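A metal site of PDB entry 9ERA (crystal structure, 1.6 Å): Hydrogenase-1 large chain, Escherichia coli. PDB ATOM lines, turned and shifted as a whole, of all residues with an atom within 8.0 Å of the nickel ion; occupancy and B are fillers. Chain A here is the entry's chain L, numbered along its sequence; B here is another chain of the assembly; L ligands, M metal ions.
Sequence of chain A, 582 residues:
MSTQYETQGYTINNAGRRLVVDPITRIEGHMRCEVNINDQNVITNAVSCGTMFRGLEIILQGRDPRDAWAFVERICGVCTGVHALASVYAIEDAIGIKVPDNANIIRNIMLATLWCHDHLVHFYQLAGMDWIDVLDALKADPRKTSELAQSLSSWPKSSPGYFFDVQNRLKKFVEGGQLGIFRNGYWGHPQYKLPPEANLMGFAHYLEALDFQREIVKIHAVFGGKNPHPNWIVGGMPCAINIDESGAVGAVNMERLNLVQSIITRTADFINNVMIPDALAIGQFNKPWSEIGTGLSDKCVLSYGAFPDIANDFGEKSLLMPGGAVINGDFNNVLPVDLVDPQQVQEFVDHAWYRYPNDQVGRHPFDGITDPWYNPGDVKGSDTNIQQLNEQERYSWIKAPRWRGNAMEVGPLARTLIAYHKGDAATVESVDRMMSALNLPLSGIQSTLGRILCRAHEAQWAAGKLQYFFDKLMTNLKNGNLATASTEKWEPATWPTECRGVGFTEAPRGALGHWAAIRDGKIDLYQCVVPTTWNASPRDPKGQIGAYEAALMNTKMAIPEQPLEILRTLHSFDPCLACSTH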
ATOM      1  N   GLU A  28     -12.402  19.897   6.402  1.00  0.00           N
ATOM      2  CA  GLU A  28     -11.609  20.969   5.825  1.00  0.00           C
ATOM      3  C   GLU A  28     -10.372  21.172   6.719  1.00  0.00           C
ATOM      4  O   GLU A  28     -10.500  21.336   7.927  1.00  0.00           O
ATOM      5  CB  GLU A  28     -12.495  22.219   5.729  1.00  0.00           C
ATOM      6  CG  GLU A  28     -11.882  23.348   4.920  1.00  0.00           C
ATOM      7  CD  GLU A  28     -10.697  23.989   5.593  1.00  0.00           C
ATOM      8  OE1 GLU A  28     -10.890  24.426   6.753  1.00  0.00           O
ATOM      9  OE2 GLU A  28      -9.590  24.019   4.979  1.00  0.00           O
ATOM     10  N   GLU A  73     -11.692  36.284   3.186  1.00  0.00           N
ATOM     11  CA  GLU A  73     -12.452  35.265   2.479  1.00  0.00           C
ATOM     12  C   GLU A  73     -11.617  33.992   2.362  1.00  0.00           C
ATOM     13  O   GLU A  73     -12.166  32.892   2.484  1.00  0.00           O
ATOM     14  CB  GLU A  73     -12.918  35.749   1.109  1.00  0.00           C
ATOM     15  CG  GLU A  73     -13.920  34.804   0.473  1.00  0.00           C
ATOM     16  CD  GLU A  73     -14.647  35.396  -0.735  1.00  0.00           C
ATOM     17  OE1 GLU A  73     -13.946  35.885  -1.653  1.00  0.00           O
ATOM     18  OE2 GLU A  73     -15.898  35.378  -0.755  1.00  0.00           O
ATOM     19  N   ILE A  75      -9.671  32.746   4.433  1.00  0.00           N
ATOM     20  CA  ILE A  75      -9.645  31.912   5.627  1.00  0.00           C
ATOM     21  C   ILE A  75     -10.157  30.519   5.258  1.00  0.00           C
ATOM     22  O   ILE A  75      -9.681  29.524   5.809  1.00  0.00           O
ATOM     23  CB  ILE A  75     -10.438  32.550   6.787  1.00  0.00           C
ATOM     24  CG1 ILE A  75      -9.699  33.760   7.374  1.00  0.00           C
ATOM     25  CG2 ILE A  75     -10.741  31.518   7.853  1.00  0.00           C
ATOM     26  CD1 ILE A  75     -10.536  34.624   8.312  1.00  0.00           C
ATOM     27  N   CYS A  76     -11.148  30.447   4.333  1.00  0.00           N
ATOM     28  CA  CYS A  76     -11.775  29.176   4.029  1.00  0.00           C
ATOM     29  C   CYS A  76     -12.466  29.190   2.671  1.00  0.00           C
ATOM     30  O   CYS A  76     -13.297  30.055   2.400  1.00  0.00           O
ATOM     31  CB  CYS A  76     -12.814  28.806   5.096  1.00  0.00           C
ATOM     32  SG  CYS A  76     -13.339  27.071   4.985  1.00  0.00           S
ATOM     33  N   GLY A  77     -12.150  28.162   1.868  1.00  0.00           N
ATOM     34  CA  GLY A  77     -12.729  27.933   0.554  1.00  0.00           C
ATOM     35  C   GLY A  77     -13.972  27.058   0.603  1.00  0.00           C
ATOM     36  O   GLY A  77     -14.656  26.915  -0.419  1.00  0.00           O
ATOM     37  N   VAL A  78     -14.239  26.458   1.779  1.00  0.00           N
ATOM     38  CA  VAL A  78     -15.410  25.614   1.982  1.00  0.00           C
ATOM     39  C   VAL A  78     -16.596  26.487   2.394  1.00  0.00           C
ATOM     40  O   VAL A  78     -17.585  26.548   1.663  1.00  0.00           O
ATOM     41  CB  VAL A  78     -15.116  24.474   2.979  1.00  0.00           C
ATOM     42  CG1 VAL A  78     -16.333  23.584   3.211  1.00  0.00           C
ATOM     43  CG2 VAL A  78     -13.944  23.628   2.518  1.00  0.00           C
ATOM     44  N   CYS A  79     -16.484  27.207   3.509  1.00  0.00           N
ATOM     45  CA  CYS A  79     -17.434  28.247   3.860  1.00  0.00           C
ATOM     46  C   CYS A  79     -17.051  29.556   3.136  1.00  0.00           C
ATOM     47  O   CYS A  79     -17.026  30.636   3.727  1.00  0.00           O
ATOM     48  CB  CYS A  79     -17.559  28.416   5.368  1.00  0.00           C
ATOM     49  SG  CYS A  79     -16.015  28.894   6.205  1.00  0.00           S
ATOM     50  N   THR A  80     -16.806  29.440   1.824  1.00  0.00           N
ATOM     51  CA  THR A  80     -16.375  30.547   0.983  1.00  0.00           C
ATOM     52  C   THR A  80     -17.432  31.642   0.932  1.00  0.00           C
ATOM     53  O   THR A  80     -18.594  31.381   0.609  1.00  0.00           O
ATOM     54  CB  THR A  80     -16.019  30.055  -0.422  1.00  0.00           C
ATOM     55  OG1 THR A  80     -15.504  31.200  -1.104  1.00  0.00           O
ATOM     56  CG2 THR A  80     -17.199  29.457  -1.168  1.00  0.00           C
ATOM     57  N   VAL A  82     -18.400  33.593   3.607  1.00  0.00           N
ATOM     58  CA  VAL A  82     -18.982  33.956   4.880  1.00  0.00           C
ATOM     59  C   VAL A  82     -18.078  34.953   5.606  1.00  0.00           C
ATOM     60  O   VAL A  82     -18.592  35.868   6.272  1.00  0.00           O
ATOM     61  CB  VAL A  82     -19.347  32.731   5.754  1.00  0.00           C
ATOM     62  CG1 VAL A  82     -18.154  32.050   6.378  1.00  0.00           C
ATOM     63  CG2 VAL A  82     -20.339  33.156   6.825  1.00  0.00           C
ATOM     64  N   HIS A  83     -16.753  34.820   5.435  1.00  0.00           N
ATOM     65  CA  HIS A  83     -15.807  35.734   6.058  1.00  0.00           C
ATOM     66  C   HIS A  83     -15.814  37.083   5.341  1.00  0.00           C
ATOM     67  O   HIS A  83     -15.569  38.123   5.955  1.00  0.00           O
ATOM     68  CB  HIS A  83     -14.386  35.123   6.095  1.00  0.00           C
ATOM     69  CG  HIS A  83     -14.270  33.961   7.011  1.00  0.00           C
ATOM     70  ND1 HIS A  83     -14.214  34.089   8.390  1.00  0.00           N
ATOM     71  CD2 HIS A  83     -14.197  32.636   6.750  1.00  0.00           C
ATOM     72  CE1 HIS A  83     -14.123  32.880   8.939  1.00  0.00           C
ATOM     73  NE2 HIS A  83     -14.111  31.980   7.964  1.00  0.00           N
ATOM     74  N   LEU A 114     -24.708  29.556   0.180  1.00  0.00           N
ATOM     75  CA  LEU A 114     -23.617  28.870   0.852  1.00  0.00           C
ATOM     76  C   LEU A 114     -24.140  27.794   1.805  1.00  0.00           C
ATOM     77  O   LEU A 114     -23.645  26.676   1.790  1.00  0.00           O
ATOM     78  CB  LEU A 114     -22.738  29.880   1.593  1.00  0.00           C
ATOM     79  CG  LEU A 114     -21.569  29.239   2.346  1.00  0.00           C
ATOM     80  CD1 LEU A 114     -20.577  28.559   1.395  1.00  0.00           C
ATOM     81  CD2 LEU A 114     -20.863  30.269   3.211  1.00  0.00           C
ATOM     82  N   ASP A 118     -22.980  24.075   1.206  1.00  0.00           N
ATOM     83  CA  ASP A 118     -22.052  23.578   2.202  1.00  0.00           C
ATOM     84  C   ASP A 118     -22.699  22.406   2.951  1.00  0.00           C
ATOM     85  O   ASP A 118     -22.084  21.355   3.132  1.00  0.00           O
ATOM     86  CB  ASP A 118     -21.626  24.752   3.078  1.00  0.00           C
ATOM     87  CG  ASP A 118     -20.351  24.525   3.877  1.00  0.00           C
ATOM     88  OD1 ASP A 118     -20.008  23.335   4.116  1.00  0.00           O
ATOM     89  OD2 ASP A 118     -19.724  25.541   4.244  1.00  0.00           O
ATOM     90  N   ALA A 507     -22.363  31.250  10.075  1.00  0.00           N
ATOM     91  CA  ALA A 507     -21.804  30.439   9.021  1.00  0.00           C
ATOM     92  C   ALA A 507     -22.418  29.053   9.094  1.00  0.00           C
ATOM     93  O   ALA A 507     -23.018  28.709  10.113  1.00  0.00           O
ATOM     94  CB  ALA A 507     -20.301  30.389   9.173  1.00  0.00           C
ATOM     95  N   PRO A 508     -22.280  28.209   8.044  1.00  0.00           N
ATOM     96  CA  PRO A 508     -22.784  26.828   8.110  1.00  0.00           C
ATOM     97  C   PRO A 508     -22.451  26.084   9.401  1.00  0.00           C
ATOM     98  O   PRO A 508     -23.284  25.316   9.892  1.00  0.00           O
ATOM     99  CB  PRO A 508     -22.173  26.169   6.861  1.00  0.00           C
ATOM    100  CG  PRO A 508     -22.040  27.320   5.880  1.00  0.00           C
ATOM    101  CD  PRO A 508     -21.701  28.540   6.736  1.00  0.00           C
ATOM    102  N   ARG A 509     -21.278  26.364   9.984  1.00  0.00           N
ATOM    103  CA  ARG A 509     -20.793  25.607  11.128  1.00  0.00           C
ATOM    104  C   ARG A 509     -21.057  26.302  12.452  1.00  0.00           C
ATOM    105  O   ARG A 509     -20.826  25.696  13.498  1.00  0.00           O
ATOM    106  CB  ARG A 509     -19.310  25.311  10.960  1.00  0.00           C
ATOM    107  CG  ARG A 509     -19.065  24.366   9.792  1.00  0.00           C
ATOM    108  CD  ARG A 509     -17.639  24.423   9.303  1.00  0.00           C
ATOM    109  NE  ARG A 509     -17.498  23.588   8.135  1.00  0.00           N
ATOM    110  CZ  ARG A 509     -17.952  23.880   6.923  1.00  0.00           C
ATOM    111  NH1 ARG A 509     -18.426  25.086   6.645  1.00  0.00           N
ATOM    112  NH2 ARG A 509     -17.895  22.947   5.980  1.00  0.00           N
ATOM    113  N   VAL A 530     -14.155  32.089  15.058  1.00  0.00           N
ATOM    114  CA  VAL A 530     -14.828  31.352  14.005  1.00  0.00           C
ATOM    115  C   VAL A 530     -15.543  30.142  14.621  1.00  0.00           C
ATOM    116  O   VAL A 530     -15.165  29.698  15.706  1.00  0.00           O
ATOM    117  CB  VAL A 530     -13.781  31.000  12.923  1.00  0.00           C
ATOM    118  CG1 VAL A 530     -14.380  30.402  11.686  1.00  0.00           C
ATOM    119  CG2 VAL A 530     -12.965  32.227  12.538  1.00  0.00           C
ATOM    120  N   PRO A 531     -16.661  29.630  14.045  1.00  0.00           N
ATOM    121  CA  PRO A 531     -17.404  28.540  14.663  1.00  0.00           C
ATOM    122  C   PRO A 531     -16.580  27.334  15.119  1.00  0.00           C
ATOM    123  O   PRO A 531     -16.765  26.859  16.233  1.00  0.00           O
ATOM    124  CB  PRO A 531     -18.444  28.105  13.611  1.00  0.00           C
ATOM    125  CG  PRO A 531     -18.311  29.060  12.472  1.00  0.00           C
ATOM    126  CD  PRO A 531     -17.367  30.159  12.884  1.00  0.00           C
ATOM    127  N   THR A 532     -15.653  26.855  14.283  1.00  0.00           N
ATOM    128  CA  THR A 532     -14.870  25.698  14.658  1.00  0.00           C
ATOM    129  C   THR A 532     -13.824  26.069  15.730  1.00  0.00           C
ATOM    130  O   THR A 532     -13.343  25.193  16.451  1.00  0.00           O
ATOM    131  CB  THR A 532     -14.271  25.002  13.428  1.00  0.00           C
ATOM    132  OG1 THR A 532     -15.328  24.623  12.547  1.00  0.00           O
ATOM    133  CG2 THR A 532     -13.472  23.768  13.782  1.00  0.00           C
ATOM    134  N   ASP A 574     -19.108  19.046  11.308  1.00  0.00           N
ATOM    135  CA  ASP A 574     -18.580  19.615  10.072  1.00  0.00           C
ATOM    136  C   ASP A 574     -17.332  20.445  10.392  1.00  0.00           C
ATOM    137  O   ASP A 574     -17.335  21.663  10.232  1.00  0.00           O
ATOM    138  CB  ASP A 574     -19.667  20.429   9.361  1.00  0.00           C
ATOM    139  CG  ASP A 574     -19.299  20.878   7.954  1.00  0.00           C
ATOM    140  OD1 ASP A 574     -18.188  20.519   7.496  1.00  0.00           O
ATOM    141  OD2 ASP A 574     -20.139  21.568   7.332  1.00  0.00           O
ATOM    142  N   PRO A 575     -16.221  19.839  10.865  1.00  0.00           N
ATOM    143  CA  PRO A 575     -15.049  20.623  11.277  1.00  0.00           C
ATOM    144  C   PRO A 575     -14.398  21.352  10.094  1.00  0.00           C
ATOM    145  O   PRO A 575     -14.126  20.733   9.054  1.00  0.00           O
ATOM    146  CB  PRO A 575     -14.110  19.562  11.883  1.00  0.00           C
ATOM    147  CG  PRO A 575     -14.995  18.383  12.168  1.00  0.00           C
ATOM    148  CD  PRO A 575     -16.018  18.388  11.040  1.00  0.00           C
ATOM    149  N   CYS A 576     -14.163  22.670  10.279  1.00  0.00           N
ATOM    150  CA  CYS A 576     -13.380  23.467   9.342  1.00  0.00           C
ATOM    151  C   CYS A 576     -12.169  24.031  10.094  1.00  0.00           C
ATOM    152  O   CYS A 576     -12.281  24.998  10.848  1.00  0.00           O
ATOM    153  CB  CYS A 576     -14.202  24.597   8.701  1.00  0.00           C
ATOM    154  SG  CYS A 576     -13.415  25.362   7.251  1.00  0.00           S
ATOM    155  N   LEU A 577     -11.011  23.389   9.891  1.00  0.00           N
ATOM    156  CA  LEU A 577      -9.840  23.653  10.719  1.00  0.00           C
ATOM    157  C   LEU A 577      -9.104  24.899  10.241  1.00  0.00           C
ATOM    158  O   LEU A 577      -8.483  25.571  11.047  1.00  0.00           O
ATOM    159  CB  LEU A 577      -8.934  22.419  10.710  1.00  0.00           C
ATOM    160  CG  LEU A 577      -9.274  21.399  11.798  1.00  0.00           C
ATOM    161  CD1 LEU A 577      -8.922  21.922  13.181  1.00  0.00           C
ATOM    162  CD2 LEU A 577     -10.756  21.010  11.757  1.00  0.00           C
ATOM    163  N   ALA A 578      -9.166  25.187   8.927  1.00  0.00           N
ATOM    164  CA  ALA A 578      -8.599  26.418   8.398  1.00  0.00           C
ATOM    165  C   ALA A 578      -9.345  27.600   9.010  1.00  0.00           C
ATOM    166  O   ALA A 578      -8.734  28.565   9.445  1.00  0.00           O
ATOM    167  CB  ALA A 578      -8.686  26.446   6.895  1.00  0.00           C
ATOM    168  N   CYS A 579     -10.674  27.521   9.048  1.00  0.00           N
ATOM    169  CA  CYS A 579     -11.495  28.493   9.754  1.00  0.00           C
ATOM    170  C   CYS A 579     -11.074  28.615  11.209  1.00  0.00           C
ATOM    171  O   CYS A 579     -10.984  29.727  11.715  1.00  0.00           O
ATOM    172  CB  CYS A 579     -12.959  28.069   9.727  1.00  0.00           C
ATOM    173  SG  CYS A 579     -13.945  28.765   8.367  1.00  0.00           S
ATOM    174  N   SER A 580     -10.898  27.472  11.892  1.00  0.00           N
ATOM    175  CA  SER A 580     -10.696  27.436  13.339  1.00  0.00           C
ATOM    176  C   SER A 580      -9.453  28.237  13.732  1.00  0.00           C
ATOM    177  O   SER A 580      -9.472  28.916  14.774  1.00  0.00           O
ATOM    178  CB  SER A 580     -10.604  26.007  13.857  1.00  0.00           C
ATOM    179  OG  SER A 580      -9.377  25.383  13.521  1.00  0.00           O
ATOM    180  N   CYS B  17      -6.845  26.845   2.275  1.00  0.00           N
ATOM    181  CA  CYS B  17      -8.201  27.145   2.658  1.00  0.00           C
ATOM    182  C   CYS B  17      -9.163  26.109   2.070  1.00  0.00           C
ATOM    183  O   CYS B  17     -10.329  26.127   2.405  1.00  0.00           O
ATOM    184  CB  CYS B  17      -8.576  28.568   2.259  1.00  0.00           C
ATOM    185  SG  CYS B  17      -9.150  28.774   0.528  1.00  0.00           S
ATOM    186  N   THR B  18      -8.655  25.231   1.186  1.00  0.00           N
ATOM    187  CA  THR B  18      -9.368  24.157   0.500  1.00  0.00           C
ATOM    188  C   THR B  18     -10.121  24.691  -0.727  1.00  0.00           C
ATOM    189  O   THR B  18     -10.933  23.974  -1.315  1.00  0.00           O
ATOM    190  CB  THR B  18     -10.223  23.328   1.480  1.00  0.00           C
ATOM    191  OG1 THR B  18      -9.384  22.933   2.572  1.00  0.00           O
ATOM    192  CG2 THR B  18     -10.808  22.068   0.872  1.00  0.00           C
HETATM  193 FE1  LIG L   1     -16.134  28.301   8.487  1.00  0.00          FE
HETATM  194  C1  LIG L   1     -16.021  27.496  10.140  1.00  0.00           C
HETATM  195  N1  LIG L   1     -15.900  26.957  11.169  1.00  0.00           N
HETATM  196  C2  LIG L   1     -17.909  27.864   8.434  1.00  0.00           C
HETATM  197  N2  LIG L   1     -19.031  27.562   8.286  1.00  0.00           N
HETATM  198  C3  LIG L   1     -16.743  29.878   9.127  1.00  0.00           C
HETATM  199  O1  LIG L   1     -17.027  30.875   9.576  1.00  0.00           O
HETATM  200 NI    NI M   1     -14.682  26.995   6.816  1.00  0.00          NI
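The side-chain sulfur (SG) of Cys 79 binds an iron atom (FE1) of the ligand, 2.4 Å away. FE1 of the ligand is bound by SG of Cys 579. N of Arg 509 is in hydrogen-bond range of N2 of the ligand (3.1 Å). A nitrogen (N2) of the ligand is in hydrogen-bond range of the guanidinium group (NH1) of Arg 509 (3.0 Å). N1 of the ligand sits at hydrogen-bond distance from N of Thr 532, at 3.1 Å. The side-chain hydroxyl of Thr 532 lies within hydrogen-bond range of a nitrogen (N1) of the ligand.
SG of Cys 576 sits close to OE1 of Glu 28, 2.7 Å away. N of Cys 576 lies within hydrogen-bond range of OG1 of Thr 532. SG of Cys 76 lies close to N of Val 78 (3.4 Å). A ring nitrogen (NE2) of His 83 lies close to the side-chain sulfur (SG) of Cys 579 (3.2 Å).
Four residues have an atom within 4 Å of the nickel ion: Cys 76, Cys 79, Cys 576 and Cys 579.
The nickel ion is bound by SG of Cys 576 (2.1 Å). The nickel ion is bound by SG of Cys 76 (2.3 Å). The nickel ion is bound by SG of Cys 79, 2.4 Å away. SG of Cys 579 is bound to the nickel ion (2.5 Å). The nickel ion has four donor atoms within binding distance.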
